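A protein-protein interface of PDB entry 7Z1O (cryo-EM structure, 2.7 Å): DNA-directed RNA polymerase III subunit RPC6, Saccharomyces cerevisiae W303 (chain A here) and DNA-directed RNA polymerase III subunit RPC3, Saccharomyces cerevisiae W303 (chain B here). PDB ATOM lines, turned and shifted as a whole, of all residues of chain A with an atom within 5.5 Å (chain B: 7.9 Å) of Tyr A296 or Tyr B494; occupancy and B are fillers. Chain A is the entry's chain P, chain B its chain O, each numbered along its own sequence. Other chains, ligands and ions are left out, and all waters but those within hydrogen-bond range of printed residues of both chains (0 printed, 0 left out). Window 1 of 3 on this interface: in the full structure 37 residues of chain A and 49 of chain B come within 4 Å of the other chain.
O of Thr B302 lies within hydrogen-bond range of N of Glu A266, at 3.3 Å. The guanidinium group (NH2) of Arg B303 lies within salt-bridge range of the side-chain carboxylate (OD2) of Asp A251 (2.6 Å). The side-chain carboxylate (OD2) of Asp A251 lies within hydrogen-bond range of the side-chain hydroxyl (OH) of Tyr B494, at 2.8 Å.
O of Leu B299 sits at hydrogen-bond distance from OG1 of Thr B302 (2.8 Å). The side-chain hydroxyl (OG) of Ser B498 lies within hydrogen-bond range of the backbone carbonyl oxygen (O) of Tyr B494, at 3.4 Å. O of Val B495 is in hydrogen-bond range of OG of Ser B498 (2.8 Å). O of Val B495 sits at hydrogen-bond distance from OG1 of Thr B499 (2.9 Å). OH of Tyr A296 sits at hydrogen-bond distance from NE2 of Gln A270, 3.3 Å away.
Among the printed residues, merely in contact across the chains: Glu A266 with Tyr B494 (3.3 Å), Phe A294 with Thr B302 (3.6 Å), Ile A293 with Val B495 (3.7 Å), Phe A294 with Tyr B494 (3.7 Å), Ile A293 with Leu B647 (3.7 Å), Tyr A296 with Ser B498 (3.7 Å), Phe A294 with Leu B299 (3.8 Å), Tyr A296 with Ala B497 (3.9 Å), Phe A294 with Val B491 (3.9 Å), Tyr A296 with Tyr B494 (3.9 Å) and Phe A294 with Ser B490 (3.97 Å).
Of the printed residues of chain B, Asp A251 touches Arg B303 (2.6 Å) and Tyr B494 (2.8 Å). Printed residues of chain B within 4 Å of Ile A293: Val B495 and Leu B647. Of the printed residues of chain A, Thr B302 touches Glu A266 (3.3 Å) and Phe A294 (3.6 Å). Of chain A, only Asp A251 (2.8 Å), Glu A266 (3.3 Å), Phe A294 (3.7 Å) and Tyr A296 (3.9 Å) come within 4 Å of Tyr B494. Of the printed residues of chain A, Ala B497 touches Tyr A296 (3.9 Å). The nearest residue of chain B that does not touch Tyr A296 is Met B505 (4.8 Å). The nearest residue of chain A that does not touch Tyr B494 is Ile A293 (4.2 Å). The nearest printed residue of chain A that does not touch Ser B490 is Ile A293 (5.6 Å).
Among the printed residues, Asp or Glu carboxylates within 4 Å of a Lys or Arg side-chain nitrogen of the other chain: Asp A251 with Arg B303.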
ATOM      1  N   ASP A 251      -0.169 -34.169 -19.972  1.00  0.00           N
ATOM      2  CA  ASP A 251      -1.212 -34.266 -18.954  1.00  0.00           C
ATOM      3  C   ASP A 251      -1.767 -35.679 -18.826  1.00  0.00           C
ATOM      4  O   ASP A 251      -2.883 -35.858 -18.325  1.00  0.00           O
ATOM      5  CB  ASP A 251      -2.358 -33.276 -19.201  1.00  0.00           C
ATOM      6  CG  ASP A 251      -3.039 -32.839 -17.919  1.00  0.00           C
ATOM      7  OD1 ASP A 251      -2.564 -33.227 -16.832  1.00  0.00           O
ATOM      8  OD2 ASP A 251      -4.049 -32.110 -17.999  1.00  0.00           O
ATOM      9  N   GLU A 266      -8.238 -37.863 -16.403  1.00  0.00           N
ATOM     10  CA  GLU A 266      -8.590 -37.355 -17.726  1.00  0.00           C
ATOM     11  C   GLU A 266      -7.986 -38.215 -18.830  1.00  0.00           C
ATOM     12  O   GLU A 266      -8.634 -38.466 -19.854  1.00  0.00           O
ATOM     13  CB  GLU A 266      -8.137 -35.902 -17.865  1.00  0.00           C
ATOM     14  CG  GLU A 266      -8.426 -35.280 -19.222  1.00  0.00           C
ATOM     15  CD  GLU A 266      -9.908 -35.151 -19.511  1.00  0.00           C
ATOM     16  OE1 GLU A 266     -10.705 -35.044 -18.554  1.00  0.00           O
ATOM     17  OE2 GLU A 266     -10.279 -35.160 -20.700  1.00  0.00           O
ATOM     18  N   GLN A 270      -9.915 -40.277 -21.707  1.00  0.00           N
ATOM     19  CA  GLN A 270      -9.636 -39.894 -23.086  1.00  0.00           C
ATOM     20  C   GLN A 270      -9.592 -41.091 -24.030  1.00  0.00           C
ATOM     21  O   GLN A 270      -9.761 -40.924 -25.243  1.00  0.00           O
ATOM     22  CB  GLN A 270      -8.318 -39.122 -23.149  1.00  0.00           C
ATOM     23  CG  GLN A 270      -8.141 -38.267 -24.389  1.00  0.00           C
ATOM     24  CD  GLN A 270      -7.107 -37.177 -24.202  1.00  0.00           C
ATOM     25  OE1 GLN A 270      -6.493 -37.062 -23.142  1.00  0.00           O
ATOM     26  NE2 GLN A 270      -6.908 -36.368 -25.236  1.00  0.00           N
ATOM     27  N   SER A 292     -18.252 -29.312 -21.506  1.00  0.00           N
ATOM     28  CA  SER A 292     -17.019 -28.922 -20.844  1.00  0.00           C
ATOM     29  C   SER A 292     -15.905 -28.919 -21.877  1.00  0.00           C
ATOM     30  O   SER A 292     -15.988 -29.622 -22.886  1.00  0.00           O
ATOM     31  CB  SER A 292     -16.674 -29.868 -19.688  1.00  0.00           C
ATOM     32  OG  SER A 292     -17.569 -29.696 -18.603  1.00  0.00           O
ATOM     33  N   ILE A 293     -14.871 -28.112 -21.632  1.00  0.00           N
ATOM     34  CA  ILE A 293     -13.758 -28.050 -22.573  1.00  0.00           C
ATOM     35  C   ILE A 293     -12.875 -29.283 -22.445  1.00  0.00           C
ATOM     36  O   ILE A 293     -12.222 -29.698 -23.411  1.00  0.00           O
ATOM     37  CB  ILE A 293     -12.962 -26.744 -22.367  1.00  0.00           C
ATOM     38  CG1 ILE A 293     -11.905 -26.570 -23.457  1.00  0.00           C
ATOM     39  CG2 ILE A 293     -12.336 -26.692 -20.980  1.00  0.00           C
ATOM     40  CD1 ILE A 293     -12.468 -26.581 -24.855  1.00  0.00           C
ATOM     41  N   PHE A 294     -12.863 -29.909 -21.267  1.00  0.00           N
ATOM     42  CA  PHE A 294     -11.922 -30.993 -21.015  1.00  0.00           C
ATOM     43  C   PHE A 294     -12.331 -32.268 -21.741  1.00  0.00           C
ATOM     44  O   PHE A 294     -11.472 -33.020 -22.215  1.00  0.00           O
ATOM     45  CB  PHE A 294     -11.803 -31.225 -19.511  1.00  0.00           C
ATOM     46  CG  PHE A 294     -11.506 -29.975 -18.735  1.00  0.00           C
ATOM     47  CD1 PHE A 294     -10.228 -29.444 -18.713  1.00  0.00           C
ATOM     48  CD2 PHE A 294     -12.509 -29.323 -18.039  1.00  0.00           C
ATOM     49  CE1 PHE A 294      -9.957 -28.292 -18.004  1.00  0.00           C
ATOM     50  CE2 PHE A 294     -12.243 -28.172 -17.330  1.00  0.00           C
ATOM     51  CZ  PHE A 294     -10.966 -27.656 -17.313  1.00  0.00           C
ATOM     52  N   ASN A 295     -13.631 -32.527 -21.845  1.00  0.00           N
ATOM     53  CA  ASN A 295     -14.126 -33.666 -22.618  1.00  0.00           C
ATOM     54  C   ASN A 295     -14.429 -33.296 -24.074  1.00  0.00           C
ATOM     55  O   ASN A 295     -15.480 -33.608 -24.633  1.00  0.00           O
ATOM     56  CB  ASN A 295     -15.319 -34.299 -21.898  1.00  0.00           C
ATOM     57  CG  ASN A 295     -16.569 -33.414 -21.858  1.00  0.00           C
ATOM     58  OD1 ASN A 295     -16.639 -32.345 -22.459  1.00  0.00           O
ATOM     59  ND2 ASN A 295     -17.574 -33.880 -21.126  1.00  0.00           N
ATOM     60  N   TYR A 296     -13.444 -32.660 -24.714  1.00  0.00           N
ATOM     61  CA  TYR A 296     -13.613 -32.184 -26.084  1.00  0.00           C
ATOM     62  C   TYR A 296     -13.604 -33.324 -27.093  1.00  0.00           C
ATOM     63  O   TYR A 296     -14.126 -33.168 -28.203  1.00  0.00           O
ATOM     64  CB  TYR A 296     -12.519 -31.173 -26.428  1.00  0.00           C
ATOM     65  CG  TYR A 296     -11.110 -31.728 -26.383  1.00  0.00           C
ATOM     66  CD1 TYR A 296     -10.400 -31.783 -25.191  1.00  0.00           C
ATOM     67  CD2 TYR A 296     -10.483 -32.182 -27.535  1.00  0.00           C
ATOM     68  CE1 TYR A 296      -9.117 -32.283 -25.145  1.00  0.00           C
ATOM     69  CE2 TYR A 296      -9.198 -32.685 -27.499  1.00  0.00           C
ATOM     70  CZ  TYR A 296      -8.521 -32.731 -26.301  1.00  0.00           C
ATOM     71  OH  TYR A 296      -7.241 -33.229 -26.257  1.00  0.00           O
ATOM     72  N   PHE A 297     -13.008 -34.466 -26.738  1.00  0.00           N
ATOM     73  CA  PHE A 297     -12.954 -35.592 -27.666  1.00  0.00           C
ATOM     74  C   PHE A 297     -14.333 -36.186 -27.914  1.00  0.00           C
ATOM     75  O   PHE A 297     -14.574 -36.776 -28.973  1.00  0.00           O
ATOM     76  CB  PHE A 297     -11.997 -36.661 -27.139  1.00  0.00           C
ATOM     77  CG  PHE A 297     -12.074 -36.865 -25.652  1.00  0.00           C
ATOM     78  CD1 PHE A 297     -13.081 -37.635 -25.095  1.00  0.00           C
ATOM     79  CD2 PHE A 297     -11.134 -36.290 -24.814  1.00  0.00           C
ATOM     80  CE1 PHE A 297     -13.151 -37.824 -23.729  1.00  0.00           C
ATOM     81  CE2 PHE A 297     -11.200 -36.475 -23.450  1.00  0.00           C
ATOM     82  CZ  PHE A 297     -12.209 -37.242 -22.906  1.00  0.00           C
ATOM     83  N   LYS A 298     -15.249 -36.044 -26.953  1.00  0.00           N
ATOM     84  CA  LYS A 298     -16.605 -36.543 -27.133  1.00  0.00           C
ATOM     85  C   LYS A 298     -17.413 -35.686 -28.099  1.00  0.00           C
ATOM     86  O   LYS A 298     -18.394 -36.175 -28.667  1.00  0.00           O
ATOM     87  CB  LYS A 298     -17.317 -36.612 -25.782  1.00  0.00           C
ATOM     88  CG  LYS A 298     -16.714 -37.611 -24.811  1.00  0.00           C
ATOM     89  CD  LYS A 298     -17.429 -37.573 -23.472  1.00  0.00           C
ATOM     90  CE  LYS A 298     -16.758 -38.488 -22.463  1.00  0.00           C
ATOM     91  NZ  LYS A 298     -17.407 -38.411 -21.125  1.00  0.00           N
ATOM     92  N   MET A 299     -17.027 -34.427 -28.291  1.00  0.00           N
ATOM     93  CA  MET A 299     -17.782 -33.531 -29.156  1.00  0.00           C
ATOM     94  C   MET A 299     -17.584 -33.899 -30.621  1.00  0.00           C
ATOM     95  O   MET A 299     -16.492 -34.297 -31.038  1.00  0.00           O
ATOM     96  CB  MET A 299     -17.356 -32.083 -28.915  1.00  0.00           C
ATOM     97  CG  MET A 299     -17.383 -31.659 -27.455  1.00  0.00           C
ATOM     98  SD  MET A 299     -19.000 -31.875 -26.688  1.00  0.00           S
ATOM     99  CE  MET A 299     -20.004 -30.796 -27.705  1.00  0.00           C
ATOM    100  N   LEU B 299     -13.862 -28.741 -13.498  1.00  0.00           N
ATOM    101  CA  LEU B 299     -12.435 -29.029 -13.383  1.00  0.00           C
ATOM    102  C   LEU B 299     -12.183 -30.219 -12.465  1.00  0.00           C
ATOM    103  O   LEU B 299     -11.326 -31.063 -12.751  1.00  0.00           O
ATOM    104  CB  LEU B 299     -11.688 -27.796 -12.880  1.00  0.00           C
ATOM    105  CG  LEU B 299     -10.187 -27.954 -12.640  1.00  0.00           C
ATOM    106  CD1 LEU B 299      -9.485 -28.395 -13.910  1.00  0.00           C
ATOM    107  CD2 LEU B 299      -9.587 -26.662 -12.119  1.00  0.00           C
ATOM    108  N   THR B 302     -12.547 -33.936 -13.735  1.00  0.00           N
ATOM    109  CA  THR B 302     -11.501 -34.524 -14.559  1.00  0.00           C
ATOM    110  C   THR B 302     -10.297 -34.991 -13.755  1.00  0.00           C
ATOM    111  O   THR B 302      -9.346 -35.516 -14.342  1.00  0.00           O
ATOM    112  CB  THR B 302     -11.041 -33.522 -15.621  1.00  0.00           C
ATOM    113  OG1 THR B 302     -10.292 -32.473 -14.998  1.00  0.00           O
ATOM    114  CG2 THR B 302     -12.243 -32.923 -16.325  1.00  0.00           C
ATOM    115  N   ARG B 303     -10.308 -34.816 -12.439  1.00  0.00           N
ATOM    116  CA  ARG B 303      -9.187 -35.223 -11.601  1.00  0.00           C
ATOM    117  C   ARG B 303      -9.561 -36.248 -10.545  1.00  0.00           C
ATOM    118  O   ARG B 303      -8.826 -37.219 -10.355  1.00  0.00           O
ATOM    119  CB  ARG B 303      -8.570 -33.998 -10.912  1.00  0.00           C
ATOM    120  CG  ARG B 303      -8.035 -32.951 -11.869  1.00  0.00           C
ATOM    121  CD  ARG B 303      -6.695 -33.356 -12.448  1.00  0.00           C
ATOM    122  NE  ARG B 303      -6.573 -32.956 -13.843  1.00  0.00           N
ATOM    123  CZ  ARG B 303      -5.435 -32.950 -14.524  1.00  0.00           C
ATOM    124  NH1 ARG B 303      -4.292 -33.305 -13.962  1.00  0.00           N
ATOM    125  NH2 ARG B 303      -5.446 -32.573 -15.799  1.00  0.00           N
ATOM    126  N   PHE B 465      -4.218 -30.488  -7.912  1.00  0.00           N
ATOM    127  CA  PHE B 465      -4.882 -29.193  -7.954  1.00  0.00           C
ATOM    128  C   PHE B 465      -5.396 -28.832  -6.561  1.00  0.00           C
ATOM    129  O   PHE B 465      -5.969 -29.681  -5.872  1.00  0.00           O
ATOM    130  CB  PHE B 465      -6.044 -29.209  -8.947  1.00  0.00           C
ATOM    131  CG  PHE B 465      -5.621 -29.277 -10.390  1.00  0.00           C
ATOM    132  CD1 PHE B 465      -4.294 -29.118 -10.754  1.00  0.00           C
ATOM    133  CD2 PHE B 465      -6.559 -29.496 -11.383  1.00  0.00           C
ATOM    134  CE1 PHE B 465      -3.912 -29.180 -12.079  1.00  0.00           C
ATOM    135  CE2 PHE B 465      -6.183 -29.558 -12.708  1.00  0.00           C
ATOM    136  CZ  PHE B 465      -4.858 -29.399 -13.057  1.00  0.00           C
ATOM    137  N   LEU B 487      -7.149 -23.137 -12.784  1.00  0.00           N
ATOM    138  CA  LEU B 487      -8.302 -23.304 -13.664  1.00  0.00           C
ATOM    139  C   LEU B 487      -8.090 -22.591 -14.995  1.00  0.00           C
ATOM    140  O   LEU B 487      -8.392 -23.141 -16.063  1.00  0.00           O
ATOM    141  CB  LEU B 487      -9.560 -22.785 -12.971  1.00  0.00           C
ATOM    142  CG  LEU B 487     -10.838 -22.702 -13.805  1.00  0.00           C
ATOM    143  CD1 LEU B 487     -11.260 -24.080 -14.275  1.00  0.00           C
ATOM    144  CD2 LEU B 487     -11.948 -22.042 -13.010  1.00  0.00           C
ATOM    145  N   LYS B 488      -7.563 -21.362 -14.945  1.00  0.00           N
ATOM    146  CA  LYS B 488      -7.297 -20.609 -16.167  1.00  0.00           C
ATOM    147  C   LYS B 488      -6.287 -21.330 -17.048  1.00  0.00           C
ATOM    148  O   LYS B 488      -6.487 -21.464 -18.263  1.00  0.00           O
ATOM    149  CB  LYS B 488      -6.791 -19.209 -15.821  1.00  0.00           C
ATOM    150  CG  LYS B 488      -7.870 -18.174 -15.587  1.00  0.00           C
ATOM    151  CD  LYS B 488      -7.273 -16.779 -15.557  1.00  0.00           C
ATOM    152  CE  LYS B 488      -7.935 -15.915 -14.503  1.00  0.00           C
ATOM    153  NZ  LYS B 488      -7.199 -14.641 -14.295  1.00  0.00           N
ATOM    154  N   SER B 489      -5.200 -21.821 -16.444  1.00  0.00           N
ATOM    155  CA  SER B 489      -4.170 -22.517 -17.205  1.00  0.00           C
ATOM    156  C   SER B 489      -4.699 -23.812 -17.806  1.00  0.00           C
ATOM    157  O   SER B 489      -4.392 -24.137 -18.957  1.00  0.00           O
ATOM    158  CB  SER B 489      -2.960 -22.793 -16.315  1.00  0.00           C
ATOM    159  OG  SER B 489      -1.992 -23.567 -16.999  1.00  0.00           O
ATOM    160  N   SER B 490      -5.498 -24.564 -17.043  1.00  0.00           N
ATOM    161  CA  SER B 490      -6.047 -25.816 -17.553  1.00  0.00           C
ATOM    162  C   SER B 490      -7.004 -25.575 -18.713  1.00  0.00           C
ATOM    163  O   SER B 490      -6.936 -26.271 -19.735  1.00  0.00           O
ATOM    164  CB  SER B 490      -6.748 -26.575 -16.429  1.00  0.00           C
ATOM    165  OG  SER B 490      -5.812 -27.259 -15.619  1.00  0.00           O
ATOM    166  N   VAL B 491      -7.893 -24.585 -18.580  1.00  0.00           N
ATOM    167  CA  VAL B 491      -8.830 -24.270 -19.656  1.00  0.00           C
ATOM    168  C   VAL B 491      -8.082 -23.805 -20.898  1.00  0.00           C
ATOM    169  O   VAL B 491      -8.391 -24.225 -22.020  1.00  0.00           O
ATOM    170  CB  VAL B 491      -9.856 -23.225 -19.179  1.00  0.00           C
ATOM    171  CG1 VAL B 491     -10.639 -22.663 -20.349  1.00  0.00           C
ATOM    172  CG2 VAL B 491     -10.801 -23.844 -18.168  1.00  0.00           C
ATOM    173  N   TYR B 492      -7.070 -22.953 -20.715  1.00  0.00           N
ATOM    174  CA  TYR B 492      -6.289 -22.446 -21.840  1.00  0.00           C
ATOM    175  C   TYR B 492      -5.538 -23.567 -22.553  1.00  0.00           C
ATOM    176  O   TYR B 492      -5.565 -23.662 -23.792  1.00  0.00           O
ATOM    177  CB  TYR B 492      -5.338 -21.371 -21.315  1.00  0.00           C
ATOM    178  CG  TYR B 492      -4.223 -20.943 -22.228  1.00  0.00           C
ATOM    179  CD1 TYR B 492      -4.440 -20.016 -23.232  1.00  0.00           C
ATOM    180  CD2 TYR B 492      -2.939 -21.428 -22.051  1.00  0.00           C
ATOM    181  CE1 TYR B 492      -3.421 -19.610 -24.056  1.00  0.00           C
ATOM    182  CE2 TYR B 492      -1.918 -21.028 -22.867  1.00  0.00           C
ATOM    183  CZ  TYR B 492      -2.159 -20.113 -23.860  1.00  0.00           C
ATOM    184  OH  TYR B 492      -1.131 -19.727 -24.680  1.00  0.00           O
ATOM    185  N   GLU B 493      -4.895 -24.450 -21.785  1.00  0.00           N
ATOM    186  CA  GLU B 493      -4.145 -25.553 -22.370  1.00  0.00           C
ATOM    187  C   GLU B 493      -5.062 -26.527 -23.094  1.00  0.00           C
ATOM    188  O   GLU B 493      -4.715 -27.032 -24.167  1.00  0.00           O
ATOM    189  CB  GLU B 493      -3.345 -26.270 -21.284  1.00  0.00           C
ATOM    190  CG  GLU B 493      -2.065 -25.555 -20.895  1.00  0.00           C
ATOM    191  CD  GLU B 493      -1.551 -25.980 -19.535  1.00  0.00           C
ATOM    192  OE1 GLU B 493      -1.914 -27.085 -19.079  1.00  0.00           O
ATOM    193  OE2 GLU B 493      -0.785 -25.209 -18.922  1.00  0.00           O
ATOM    194  N   TYR B 494      -6.247 -26.794 -22.541  1.00  0.00           N
ATOM    195  CA  TYR B 494      -7.145 -27.726 -23.211  1.00  0.00           C
ATOM    196  C   TYR B 494      -7.814 -27.109 -24.432  1.00  0.00           C
ATOM    197  O   TYR B 494      -8.117 -27.830 -25.388  1.00  0.00           O
ATOM    198  CB  TYR B 494      -8.185 -28.258 -22.228  1.00  0.00           C
ATOM    199  CG  TYR B 494      -7.694 -29.479 -21.490  1.00  0.00           C
ATOM    200  CD1 TYR B 494      -6.588 -29.407 -20.658  1.00  0.00           C
ATOM    201  CD2 TYR B 494      -8.319 -30.707 -21.643  1.00  0.00           C
ATOM    202  CE1 TYR B 494      -6.125 -30.516 -19.987  1.00  0.00           C
ATOM    203  CE2 TYR B 494      -7.862 -31.824 -20.974  1.00  0.00           C
ATOM    204  CZ  TYR B 494      -6.765 -31.721 -20.149  1.00  0.00           C
ATOM    205  OH  TYR B 494      -6.301 -32.827 -19.478  1.00  0.00           O
ATOM    206  N   VAL B 495      -8.028 -25.790 -24.441  1.00  0.00           N
ATOM    207  CA  VAL B 495      -8.497 -25.135 -25.660  1.00  0.00           C
ATOM    208  C   VAL B 495      -7.446 -25.256 -26.756  1.00  0.00           C
ATOM    209  O   VAL B 495      -7.764 -25.573 -27.912  1.00  0.00           O
ATOM    210  CB  VAL B 495      -8.862 -23.665 -25.386  1.00  0.00           C
ATOM    211  CG1 VAL B 495      -8.932 -22.889 -26.682  1.00  0.00           C
ATOM    212  CG2 VAL B 495     -10.180 -23.570 -24.654  1.00  0.00           C
ATOM    213  N   ILE B 496      -6.175 -25.023 -26.408  1.00  0.00           N
ATOM    214  CA  ILE B 496      -5.104 -25.188 -27.392  1.00  0.00           C
ATOM    215  C   ILE B 496      -5.010 -26.638 -27.855  1.00  0.00           C
ATOM    216  O   ILE B 496      -4.757 -26.911 -29.033  1.00  0.00           O
ATOM    217  CB  ILE B 496      -3.765 -24.686 -26.826  1.00  0.00           C
ATOM    218  CG1 ILE B 496      -3.817 -23.188 -26.590  1.00  0.00           C
ATOM    219  CG2 ILE B 496      -2.628 -24.971 -27.770  1.00  0.00           C
ATOM    220  CD1 ILE B 496      -2.599 -22.702 -25.907  1.00  0.00           C
ATOM    221  N   ALA B 497      -5.216 -27.587 -26.942  1.00  0.00           N
ATOM    222  CA  ALA B 497      -5.200 -28.996 -27.323  1.00  0.00           C
ATOM    223  C   ALA B 497      -6.316 -29.321 -28.302  1.00  0.00           C
ATOM    224  O   ALA B 497      -6.109 -30.058 -29.272  1.00  0.00           O
ATOM    225  CB  ALA B 497      -5.327 -29.870 -26.084  1.00  0.00           C
ATOM    226  N   SER B 498      -7.508 -28.783 -28.061  1.00  0.00           N
ATOM    227  CA  SER B 498      -8.636 -29.046 -28.940  1.00  0.00           C
ATOM    228  C   SER B 498      -8.482 -28.369 -30.294  1.00  0.00           C
ATOM    229  O   SER B 498      -8.975 -28.892 -31.299  1.00  0.00           O
ATOM    230  CB  SER B 498      -9.929 -28.589 -28.272  1.00  0.00           C
ATOM    231  OG  SER B 498      -9.990 -27.176 -28.189  1.00  0.00           O
ATOM    232  N   THR B 499      -7.813 -27.218 -30.347  1.00  0.00           N
ATOM    233  CA  THR B 499      -7.700 -26.486 -31.606  1.00  0.00           C
ATOM    234  C   THR B 499      -6.448 -26.868 -32.395  1.00  0.00           C
ATOM    235  O   THR B 499      -6.546 -27.379 -33.514  1.00  0.00           O
ATOM    236  CB  THR B 499      -7.720 -24.977 -31.336  1.00  0.00           C
ATOM    237  OG1 THR B 499      -6.679 -24.640 -30.411  1.00  0.00           O
ATOM    238  CG2 THR B 499      -9.060 -24.565 -30.755  1.00  0.00           C
ATOM    239  N   LEU B 500      -5.269 -26.636 -31.822  1.00  0.00           N
ATOM    240  CA  LEU B 500      -4.008 -26.837 -32.522  1.00  0.00           C
ATOM    241  C   LEU B 500      -3.419 -28.231 -32.343  1.00  0.00           C
ATOM    242  O   LEU B 500      -2.432 -28.555 -33.012  1.00  0.00           O
ATOM    243  CB  LEU B 500      -2.981 -25.798 -32.057  1.00  0.00           C
ATOM    244  CG  LEU B 500      -3.368 -24.332 -32.238  1.00  0.00           C
ATOM    245  CD1 LEU B 500      -2.379 -23.429 -31.529  1.00  0.00           C
ATOM    246  CD2 LEU B 500      -3.450 -23.983 -33.712  1.00  0.00           C
ATOM    247  N   GLY B 501      -3.985 -29.059 -31.469  1.00  0.00           N
ATOM    248  CA  GLY B 501      -3.518 -30.415 -31.302  1.00  0.00           C
ATOM    249  C   GLY B 501      -2.887 -30.682 -29.951  1.00  0.00           C
ATOM    250  O   GLY B 501      -2.475 -29.762 -29.237  1.00  0.00           O
ATOM    251  N   PRO B 502      -2.824 -31.960 -29.562  1.00  0.00           N
ATOM    252  CA  PRO B 502      -2.166 -32.314 -28.292  1.00  0.00           C
ATOM    253  C   PRO B 502      -0.681 -31.994 -28.259  1.00  0.00           C
ATOM    254  O   PRO B 502      -0.138 -31.718 -27.179  1.00  0.00           O
ATOM    255  CB  PRO B 502      -2.423 -33.823 -28.177  1.00  0.00           C
ATOM    256  CG  PRO B 502      -2.672 -34.277 -29.575  1.00  0.00           C
ATOM    257  CD  PRO B 502      -3.357 -33.139 -30.263  1.00  0.00           C
ATOM    258  N   MET B 505      -0.312 -28.692 -26.809  1.00  0.00           N
ATOM    259  CA  MET B 505      -0.343 -28.755 -25.348  1.00  0.00           C
ATOM    260  C   MET B 505       1.015 -29.149 -24.794  1.00  0.00           C
ATOM    261  O   MET B 505       1.500 -28.558 -23.820  1.00  0.00           O
ATOM    262  CB  MET B 505      -1.375 -29.768 -24.847  1.00  0.00           C
ATOM    263  CG  MET B 505      -1.693 -29.556 -23.368  1.00  0.00           C
ATOM    264  SD  MET B 505      -2.449 -30.906 -22.431  1.00  0.00           S
ATOM    265  CE  MET B 505      -3.580 -31.640 -23.591  1.00  0.00           C
ATOM    266  N   ARG B 509       3.224 -26.667 -22.422  1.00  0.00           N
ATOM    267  CA  ARG B 509       3.539 -27.044 -21.048  1.00  0.00           C
ATOM    268  C   ARG B 509       5.033 -27.273 -20.855  1.00  0.00           C
ATOM    269  O   ARG B 509       5.560 -27.015 -19.765  1.00  0.00           O
ATOM    270  CB  ARG B 509       2.743 -28.285 -20.651  1.00  0.00           C
ATOM    271  CG  ARG B 509       1.329 -27.969 -20.199  1.00  0.00           C
ATOM    272  CD  ARG B 509       0.485 -29.222 -20.077  1.00  0.00           C
ATOM    273  NE  ARG B 509       0.764 -29.947 -18.846  1.00  0.00           N
ATOM    274  CZ  ARG B 509       0.075 -29.806 -17.723  1.00  0.00           C
ATOM    275  NH1 ARG B 509      -0.956 -28.980 -17.645  1.00  0.00           N
ATOM    276  NH2 ARG B 509       0.427 -30.512 -16.652  1.00  0.00           N
ATOM    277  N   MET B 577      -6.708 -14.631 -25.842  1.00  0.00           N
ATOM    278  CA  MET B 577      -7.790 -15.587 -26.042  1.00  0.00           C
ATOM    279  C   MET B 577      -9.120 -15.030 -25.546  1.00  0.00           C
ATOM    280  O   MET B 577     -10.170 -15.331 -26.121  1.00  0.00           O
ATOM    281  CB  MET B 577      -7.478 -16.922 -25.372  1.00  0.00           C
ATOM    282  CG  MET B 577      -8.500 -17.974 -25.759  1.00  0.00           C
ATOM    283  SD  MET B 577      -7.823 -19.609 -26.033  1.00  0.00           S
ATOM    284  CE  MET B 577      -7.693 -20.200 -24.361  1.00  0.00           C
ATOM    285  N   LEU B 647     -16.696 -20.861 -21.845  1.00  0.00           N
ATOM    286  CA  LEU B 647     -15.270 -20.885 -22.133  1.00  0.00           C
ATOM    287  C   LEU B 647     -14.603 -19.524 -21.976  1.00  0.00           C
ATOM    288  O   LEU B 647     -13.371 -19.459 -21.927  1.00  0.00           O
ATOM    289  CB  LEU B 647     -15.048 -21.401 -23.559  1.00  0.00           C
ATOM    290  CG  LEU B 647     -13.725 -22.084 -23.880  1.00  0.00           C
ATOM    291  CD1 LEU B 647     -13.429 -23.130 -22.830  1.00  0.00           C
ATOM    292  CD2 LEU B 647     -13.791 -22.714 -25.255  1.00  0.00           C
